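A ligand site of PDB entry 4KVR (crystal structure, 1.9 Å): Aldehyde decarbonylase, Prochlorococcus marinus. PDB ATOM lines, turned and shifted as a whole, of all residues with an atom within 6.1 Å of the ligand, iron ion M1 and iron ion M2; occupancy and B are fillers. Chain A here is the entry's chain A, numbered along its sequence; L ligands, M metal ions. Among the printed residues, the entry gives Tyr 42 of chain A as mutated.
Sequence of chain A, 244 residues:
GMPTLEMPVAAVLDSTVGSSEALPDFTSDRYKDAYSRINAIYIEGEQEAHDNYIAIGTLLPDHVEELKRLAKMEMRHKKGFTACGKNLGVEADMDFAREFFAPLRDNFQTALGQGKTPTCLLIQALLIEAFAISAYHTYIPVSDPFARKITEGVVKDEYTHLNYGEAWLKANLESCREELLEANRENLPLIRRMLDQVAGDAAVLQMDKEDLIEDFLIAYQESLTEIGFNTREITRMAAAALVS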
ATOM      1  N   ILE A  41     -32.188   0.195  17.897  1.00  0.00           N
ATOM      2  CA  ILE A  41     -31.228   0.804  16.976  1.00  0.00           C
ATOM      3  C   ILE A  41     -29.817   0.810  17.593  1.00  0.00           C
ATOM      4  O   ILE A  41     -28.851   0.439  16.919  1.00  0.00           O
ATOM      5  CB  ILE A  41     -31.707   2.180  16.517  1.00  0.00           C
ATOM      6  CG1 ILE A  41     -32.860   2.007  15.522  1.00  0.00           C
ATOM      7  CG2 ILE A  41     -30.537   2.987  15.892  1.00  0.00           C
ATOM      8  CD1 ILE A  41     -33.642   3.287  15.265  1.00  0.00           C
ATOM      9  N   TYR A  42     -29.708   1.189  18.868  1.00  0.00           N
ATOM     10  CA  TYR A  42     -28.426   1.134  19.560  1.00  0.00           C
ATOM     11  C   TYR A  42     -27.837  -0.282  19.483  1.00  0.00           C
ATOM     12  O   TYR A  42     -26.704  -0.479  19.054  1.00  0.00           O
ATOM     13  CB  TYR A  42     -28.577   1.525  21.027  1.00  0.00           C
ATOM     14  CG  TYR A  42     -29.030   2.951  21.301  1.00  0.00           C
ATOM     15  CD1 TYR A  42     -29.051   3.917  20.299  1.00  0.00           C
ATOM     16  CD2 TYR A  42     -29.426   3.319  22.574  1.00  0.00           C
ATOM     17  CE1 TYR A  42     -29.464   5.214  20.577  1.00  0.00           C
ATOM     18  CE2 TYR A  42     -29.837   4.601  22.860  1.00  0.00           C
ATOM     19  CZ  TYR A  42     -29.859   5.544  21.865  1.00  0.00           C
ATOM     20  OH  TYR A  42     -30.274   6.816  22.191  1.00  0.00           O
ATOM     21  N   ILE A  43     -28.629  -1.267  19.907  1.00  0.00           N
ATOM     22  CA  ILE A  43     -28.178  -2.657  19.927  1.00  0.00           C
ATOM     23  C   ILE A  43     -27.747  -3.152  18.548  1.00  0.00           C
ATOM     24  O   ILE A  43     -26.640  -3.687  18.386  1.00  0.00           O
ATOM     25  CB  ILE A  43     -29.255  -3.577  20.511  1.00  0.00           C
ATOM     26  CG1 ILE A  43     -29.458  -3.237  21.995  1.00  0.00           C
ATOM     27  CG2 ILE A  43     -28.846  -5.032  20.356  1.00  0.00           C
ATOM     28  CD1 ILE A  43     -30.725  -3.861  22.585  1.00  0.00           C
ATOM     29  N   GLU A  44     -28.593  -2.943  17.549  1.00  0.00           N
ATOM     30  CA  GLU A  44     -28.271  -3.391  16.195  1.00  0.00           C
ATOM     31  C   GLU A  44     -27.046  -2.664  15.650  1.00  0.00           C
ATOM     32  O   GLU A  44     -26.228  -3.252  14.932  1.00  0.00           O
ATOM     33  CB  GLU A  44     -29.463  -3.208  15.255  1.00  0.00           C
ATOM     34  CG  GLU A  44     -29.220  -3.640  13.802  1.00  0.00           C
ATOM     35  CD  GLU A  44     -28.986  -5.126  13.647  1.00  0.00           C
ATOM     36  OE1 GLU A  44     -29.322  -5.905  14.570  1.00  0.00           O
ATOM     37  OE2 GLU A  44     -28.449  -5.551  12.604  1.00  0.00           O
ATOM     38  N   GLY A  45     -26.925  -1.383  15.988  1.00  0.00           N
ATOM     39  CA  GLY A  45     -25.816  -0.568  15.525  1.00  0.00           C
ATOM     40  C   GLY A  45     -24.496  -1.114  16.053  1.00  0.00           C
ATOM     41  O   GLY A  45     -23.526  -1.222  15.316  1.00  0.00           O
ATOM     42  N   GLU A  46     -24.482  -1.466  17.324  1.00  0.00           N
ATOM     43  CA  GLU A  46     -23.279  -2.046  17.935  1.00  0.00           C
ATOM     44  C   GLU A  46     -22.952  -3.389  17.290  1.00  0.00           C
ATOM     45  O   GLU A  46     -21.803  -3.659  16.972  1.00  0.00           O
ATOM     46  CB  GLU A  46     -23.458  -2.216  19.449  1.00  0.00           C
ATOM     47  CG  GLU A  46     -23.785  -0.944  20.222  1.00  0.00           C
ATOM     48  CD  GLU A  46     -22.714   0.120  20.097  1.00  0.00           C
ATOM     49  OE1 GLU A  46     -21.563  -0.216  19.736  1.00  0.00           O
ATOM     50  OE2 GLU A  46     -23.020   1.292  20.390  1.00  0.00           O
ATOM     51  N   ALA A  49     -21.507  -2.815  13.792  1.00  0.00           N
ATOM     52  CA  ALA A  49     -20.164  -2.267  13.952  1.00  0.00           C
ATOM     53  C   ALA A  49     -19.161  -3.396  14.201  1.00  0.00           C
ATOM     54  O   ALA A  49     -18.117  -3.470  13.549  1.00  0.00           O
ATOM     55  CB  ALA A  49     -20.142  -1.240  15.080  1.00  0.00           C
ATOM     56  N   TYR A  53     -16.120  -4.218  11.505  1.00  0.00           N
ATOM     57  CA  TYR A  53     -14.701  -4.238  11.822  1.00  0.00           C
ATOM     58  C   TYR A  53     -14.050  -5.599  11.518  1.00  0.00           C
ATOM     59  O   TYR A  53     -12.944  -5.643  10.987  1.00  0.00           O
ATOM     60  CB  TYR A  53     -14.457  -3.771  13.263  1.00  0.00           C
ATOM     61  CG  TYR A  53     -14.671  -2.285  13.425  1.00  0.00           C
ATOM     62  CD1 TYR A  53     -14.000  -1.397  12.592  1.00  0.00           C
ATOM     63  CD2 TYR A  53     -15.570  -1.773  14.360  1.00  0.00           C
ATOM     64  CE1 TYR A  53     -14.190  -0.029  12.710  1.00  0.00           C
ATOM     65  CE2 TYR A  53     -15.778  -0.396  14.474  1.00  0.00           C
ATOM     66  CZ  TYR A  53     -15.071   0.467  13.637  1.00  0.00           C
ATOM     67  OH  TYR A  53     -15.244   1.828  13.718  1.00  0.00           O
ATOM     68  N   MET A  73     -14.942  -4.363  21.560  1.00  0.00           N
ATOM     69  CA  MET A  73     -15.506  -3.222  22.263  1.00  0.00           C
ATOM     70  C   MET A  73     -16.964  -3.047  21.852  1.00  0.00           C
ATOM     71  O   MET A  73     -17.807  -2.761  22.682  1.00  0.00           O
ATOM     72  CB  MET A  73     -14.767  -1.911  21.939  1.00  0.00           C
ATOM     73  CG  MET A  73     -13.270  -1.906  22.179  1.00  0.00           C
ATOM     74  SD  MET A  73     -12.528  -0.314  21.699  1.00  0.00           S
ATOM     75  CE  MET A  73     -13.726   0.777  22.435  1.00  0.00           C
ATOM     76  N   GLU A  74     -17.233  -3.223  20.556  1.00  0.00           N
ATOM     77  CA  GLU A  74     -18.598  -3.062  20.068  1.00  0.00           C
ATOM     78  C   GLU A  74     -19.529  -4.071  20.718  1.00  0.00           C
ATOM     79  O   GLU A  74     -20.697  -3.777  20.981  1.00  0.00           O
ATOM     80  CB  GLU A  74     -18.661  -3.194  18.539  1.00  0.00           C
ATOM     81  CG  GLU A  74     -17.772  -2.198  17.765  1.00  0.00           C
ATOM     82  CD  GLU A  74     -18.201  -0.736  17.882  1.00  0.00           C
ATOM     83  OE1 GLU A  74     -18.936  -0.364  18.806  1.00  0.00           O
ATOM     84  OE2 GLU A  74     -17.776   0.070  17.016  1.00  0.00           O
ATOM     85  N   HIS A  77     -20.392  -2.824  24.073  1.00  0.00           N
ATOM     86  CA  HIS A  77     -21.391  -1.772  23.930  1.00  0.00           C
ATOM     87  C   HIS A  77     -22.782  -2.407  23.750  1.00  0.00           C
ATOM     88  O   HIS A  77     -23.751  -1.951  24.330  1.00  0.00           O
ATOM     89  CB  HIS A  77     -21.069  -0.906  22.696  1.00  0.00           C
ATOM     90  CG  HIS A  77     -19.802  -0.112  22.807  1.00  0.00           C
ATOM     91  ND1 HIS A  77     -19.233   0.543  21.730  1.00  0.00           N
ATOM     92  CD2 HIS A  77     -19.006   0.160  23.870  1.00  0.00           C
ATOM     93  CE1 HIS A  77     -18.135   1.162  22.128  1.00  0.00           C
ATOM     94  NE2 HIS A  77     -17.980   0.950  23.417  1.00  0.00           N
ATOM     95  N   PHE A 101     -31.179  -0.005   9.422  1.00  0.00           N
ATOM     96  CA  PHE A 101     -29.781  -0.066   9.009  1.00  0.00           C
ATOM     97  C   PHE A 101     -29.592  -0.673   7.616  1.00  0.00           C
ATOM     98  O   PHE A 101     -28.494  -0.644   7.073  1.00  0.00           O
ATOM     99  CB  PHE A 101     -28.930  -0.829  10.026  1.00  0.00           C
ATOM    100  CG  PHE A 101     -28.522  -0.007  11.218  1.00  0.00           C
ATOM    101  CD1 PHE A 101     -27.556   0.977  11.088  1.00  0.00           C
ATOM    102  CD2 PHE A 101     -29.129  -0.187  12.437  1.00  0.00           C
ATOM    103  CE1 PHE A 101     -27.189   1.755  12.185  1.00  0.00           C
ATOM    104  CE2 PHE A 101     -28.762   0.597  13.545  1.00  0.00           C
ATOM    105  CZ  PHE A 101     -27.794   1.560  13.412  1.00  0.00           C
ATOM    106  N   GLN A 124     -18.352   2.887   7.979  1.00  0.00           N
ATOM    107  CA  GLN A 124     -18.349   2.420   9.388  1.00  0.00           C
ATOM    108  C   GLN A 124     -17.607   3.343  10.358  1.00  0.00           C
ATOM    109  O   GLN A 124     -18.193   3.835  11.319  1.00  0.00           O
ATOM    110  CB  GLN A 124     -17.782   1.004   9.528  1.00  0.00           C
ATOM    111  CG  GLN A 124     -17.612   0.572  11.010  1.00  0.00           C
ATOM    112  CD  GLN A 124     -18.923   0.580  11.786  1.00  0.00           C
ATOM    113  OE1 GLN A 124     -19.939   0.065  11.304  1.00  0.00           O
ATOM    114  NE2 GLN A 124     -18.913   1.166  12.986  1.00  0.00           N
ATOM    115  N   ILE A 128     -21.064   6.001  10.524  1.00  0.00           N
ATOM    116  CA  ILE A 128     -21.768   5.298  11.601  1.00  0.00           C
ATOM    117  C   ILE A 128     -21.237   5.676  12.997  1.00  0.00           C
ATOM    118  O   ILE A 128     -22.025   5.859  13.915  1.00  0.00           O
ATOM    119  CB  ILE A 128     -21.768   3.774  11.361  1.00  0.00           C
ATOM    120  CG1 ILE A 128     -22.763   3.439  10.253  1.00  0.00           C
ATOM    121  CG2 ILE A 128     -22.185   3.022  12.602  1.00  0.00           C
ATOM    122  CD1 ILE A 128     -22.636   2.034   9.743  1.00  0.00           C
ATOM    123  N   GLU A 129     -19.924   5.816  13.144  1.00  0.00           N
ATOM    124  CA  GLU A 129     -19.391   6.258  14.434  1.00  0.00           C
ATOM    125  C   GLU A 129     -19.843   7.675  14.771  1.00  0.00           C
ATOM    126  O   GLU A 129     -20.196   7.942  15.914  1.00  0.00           O
ATOM    127  CB  GLU A 129     -17.860   6.168  14.499  1.00  0.00           C
ATOM    128  CG  GLU A 129     -17.317   4.776  14.293  1.00  0.00           C
ATOM    129  CD  GLU A 129     -17.590   3.809  15.462  1.00  0.00           C
ATOM    130  OE1 GLU A 129     -18.027   4.234  16.560  1.00  0.00           O
ATOM    131  OE2 GLU A 129     -17.317   2.605  15.281  1.00  0.00           O
ATOM    132  N   PHE A 131     -22.593   9.050  13.736  1.00  0.00           N
ATOM    133  CA  PHE A 131     -24.026   8.963  14.017  1.00  0.00           C
ATOM    134  C   PHE A 131     -24.196   8.487  15.462  1.00  0.00           C
ATOM    135  O   PHE A 131     -25.049   8.992  16.208  1.00  0.00           O
ATOM    136  CB  PHE A 131     -24.686   7.996  13.046  1.00  0.00           C
ATOM    137  CG  PHE A 131     -26.149   7.800  13.288  1.00  0.00           C
ATOM    138  CD1 PHE A 131     -27.074   8.753  12.855  1.00  0.00           C
ATOM    139  CD2 PHE A 131     -26.616   6.679  13.960  1.00  0.00           C
ATOM    140  CE1 PHE A 131     -28.436   8.574  13.091  1.00  0.00           C
ATOM    141  CE2 PHE A 131     -27.973   6.494  14.208  1.00  0.00           C
ATOM    142  CZ  PHE A 131     -28.886   7.445  13.767  1.00  0.00           C
ATOM    143  N   ALA A 132     -23.358   7.531  15.834  1.00  0.00           N
ATOM    144  CA  ALA A 132     -23.392   6.952  17.180  1.00  0.00           C
ATOM    145  C   ALA A 132     -23.057   8.000  18.236  1.00  0.00           C
ATOM    146  O   ALA A 132     -23.792   8.180  19.203  1.00  0.00           O
ATOM    147  CB  ALA A 132     -22.432   5.795  17.282  1.00  0.00           C
ATOM    148  N   ALA A 135     -25.891  10.489  18.627  1.00  0.00           N
ATOM    149  CA  ALA A 135     -27.024   9.893  19.321  1.00  0.00           C
ATOM    150  C   ALA A 135     -26.724   9.756  20.800  1.00  0.00           C
ATOM    151  O   ALA A 135     -27.531  10.131  21.657  1.00  0.00           O
ATOM    152  CB  ALA A 135     -27.332   8.537  18.737  1.00  0.00           C
ATOM    153  N   TYR A 136     -25.554   9.202  21.104  1.00  0.00           N
ATOM    154  CA  TYR A 136     -25.198   8.922  22.504  1.00  0.00           C
ATOM    155  C   TYR A 136     -24.956  10.207  23.300  1.00  0.00           C
ATOM    156  O   TYR A 136     -25.452  10.349  24.416  1.00  0.00           O
ATOM    157  CB  TYR A 136     -24.012   7.962  22.576  1.00  0.00           C
ATOM    158  CG  TYR A 136     -24.317   6.592  22.001  1.00  0.00           C
ATOM    159  CD1 TYR A 136     -25.588   6.066  22.082  1.00  0.00           C
ATOM    160  CD2 TYR A 136     -23.332   5.832  21.375  1.00  0.00           C
ATOM    161  CE1 TYR A 136     -25.889   4.833  21.563  1.00  0.00           C
ATOM    162  CE2 TYR A 136     -23.632   4.569  20.841  1.00  0.00           C
ATOM    163  CZ  TYR A 136     -24.921   4.088  20.945  1.00  0.00           C
ATOM    164  OH  TYR A 136     -25.268   2.844  20.451  1.00  0.00           O
ATOM    165  N   VAL A 154     -19.642   4.487  26.890  1.00  0.00           N
ATOM    166  CA  VAL A 154     -19.626   4.216  25.461  1.00  0.00           C
ATOM    167  C   VAL A 154     -19.065   5.371  24.624  1.00  0.00           C
ATOM    168  O   VAL A 154     -18.246   5.147  23.731  1.00  0.00           O
ATOM    169  CB  VAL A 154     -21.037   3.818  24.961  1.00  0.00           C
ATOM    170  CG1 VAL A 154     -21.073   3.765  23.433  1.00  0.00           C
ATOM    171  CG2 VAL A 154     -21.453   2.468  25.548  1.00  0.00           C
ATOM    172  N   ASP A 157     -15.436   5.745  24.022  1.00  0.00           N
ATOM    173  CA  ASP A 157     -14.922   4.712  23.139  1.00  0.00           C
ATOM    174  C   ASP A 157     -15.061   5.020  21.657  1.00  0.00           C
ATOM    175  O   ASP A 157     -14.214   4.659  20.848  1.00  0.00           O
ATOM    176  CB  ASP A 157     -15.637   3.404  23.419  1.00  0.00           C
ATOM    177  CG  ASP A 157     -15.205   2.777  24.722  1.00  0.00           C
ATOM    178  OD1 ASP A 157     -14.061   3.047  25.143  1.00  0.00           O
ATOM    179  OD2 ASP A 157     -16.005   2.035  25.312  1.00  0.00           O
ATOM    180  N   GLU A 158     -16.163   5.642  21.259  1.00  0.00           N
ATOM    181  CA  GLU A 158     -16.382   5.734  19.822  1.00  0.00           C
ATOM    182  C   GLU A 158     -15.440   6.762  19.167  1.00  0.00           C
ATOM    183  O   GLU A 158     -15.198   6.712  17.969  1.00  0.00           O
ATOM    184  CB  GLU A 158     -17.883   5.897  19.469  1.00  0.00           C
ATOM    185  CG  GLU A 158     -18.866   5.058  20.365  1.00  0.00           C
ATOM    186  CD  GLU A 158     -19.144   3.573  19.952  1.00  0.00           C
ATOM    187  OE1 GLU A 158     -18.324   2.877  19.291  1.00  0.00           O
ATOM    188  OE2 GLU A 158     -20.228   3.059  20.344  1.00  0.00           O
ATOM    189  N   HIS A 161     -12.726   4.849  17.793  1.00  0.00           N
ATOM    190  CA  HIS A 161     -13.104   4.270  16.533  1.00  0.00           C
ATOM    191  C   HIS A 161     -12.969   5.303  15.403  1.00  0.00           C
ATOM    192  O   HIS A 161     -12.448   4.979  14.339  1.00  0.00           O
ATOM    193  CB  HIS A 161     -14.519   3.709  16.624  1.00  0.00           C
ATOM    194  CG  HIS A 161     -14.667   2.651  17.671  1.00  0.00           C
ATOM    195  ND1 HIS A 161     -15.864   2.005  17.907  1.00  0.00           N
ATOM    196  CD2 HIS A 161     -13.776   2.136  18.550  1.00  0.00           C
ATOM    197  CE1 HIS A 161     -15.702   1.134  18.887  1.00  0.00           C
ATOM    198  NE2 HIS A 161     -14.441   1.192  19.302  1.00  0.00           N
HETATM  199  C1  LIG L   1     -22.407   2.060  15.852  1.00  0.00           C
HETATM  200  C2  LIG L   1     -21.086   1.989  16.543  1.00  0.00           C
HETATM  201  O1  LIG L   1     -21.057   1.736  17.762  1.00  0.00           O
HETATM  202  C3  LIG L   1     -23.515   2.403  16.805  1.00  0.00           C
HETATM  203  C4  LIG L   1     -24.581   3.150  16.054  1.00  0.00           C
HETATM  204  C5  LIG L   1     -25.891   3.031  16.767  1.00  0.00           C
HETATM  205  C6  LIG L   1     -26.542   4.366  16.895  1.00  0.00           C
HETATM  206  O2  LIG L   1     -20.010   2.194  15.926  1.00  0.00           O
HETATM  207 FE    FE M   1     -19.970   1.056  19.684  1.00  0.00          FE
HETATM  208 FE    FE M   2     -17.956   2.077  17.297  1.00  0.00          FE
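The side-chain amide nitrogen (NE2) of Gln 124 sits close to an oxygen (O2) of the ligand (3.3 Å).
The side-chain sulfur (SD) of Met 73 lies close to a ring nitrogen (NE2) of His 161, 3.4 Å away. The backbone carbonyl oxygen (O) of Gln 124 is in hydrogen-bond range of the backbone NH (N) of Glu 129 (3.2 Å). A ring nitrogen (NE2) of His 77 lies within hydrogen-bond range of the side-chain carboxylate (OD2) of Asp 157. The side-chain carboxylate of Glu 129 sits close to the side-chain hydroxyl of Tyr 53. The side-chain hydroxyl (OH) of Tyr 136 lies within hydrogen-bond range of the side-chain carboxylate (OE2) of Glu 46 (2.7 Å).
O of Ile 41 touches C5 of the ligand, 3.9 Å away. Gly 45 touches the ligand. Ala 49 touches the ligand (CB to O2, 3.5 Å). Ile 128 touches the ligand (CG2 to C1, 3.4 Å). Phe 131 touches the ligand. Ala 132 touches the ligand. Tyr 136 touches the ligand (OH to C5, 3.7 Å). Hydrophobic or aromatic side chains within 4 Å of the ligand: Ala 49, Ile 128, Phe 131 and Ala 132. 12 residues have an atom within 4 Å of the ligand: Ile 41, Gly 45, Glu 46, Ala 49, Glu 74, Gln 124, Ile 128, Glu 129, Phe 131, Ala 132, Tyr 136 and Glu 158.
Of the 23 residues printed, 4 come within 4 Å of iron ion M1. The nearest printed residue that does not touch iron ion M1 is His 161 (4.3 Å).
Of the 23 residues printed, 4 come within 4 Å of iron ion M2.
Iron ion M1 is bound by OE1 of Glu 74, OE1 of Glu 46, OE2 of Glu 158, ND1 of His 77, O1 of the ligand and OE1 of Glu 158.
Iron ion M2 is bound by OE2 of Glu 74 (2.0 Å), OE2 of Glu 129 (2.2 Å), ND1 of His 161 (2.2 Å), OE1 of Glu 158 (2.2 Å), OE1 of Glu 129 (2.3 Å) and O2 of the ligand (2.5 Å). Iron ion M2 has six donor atoms within binding distance.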
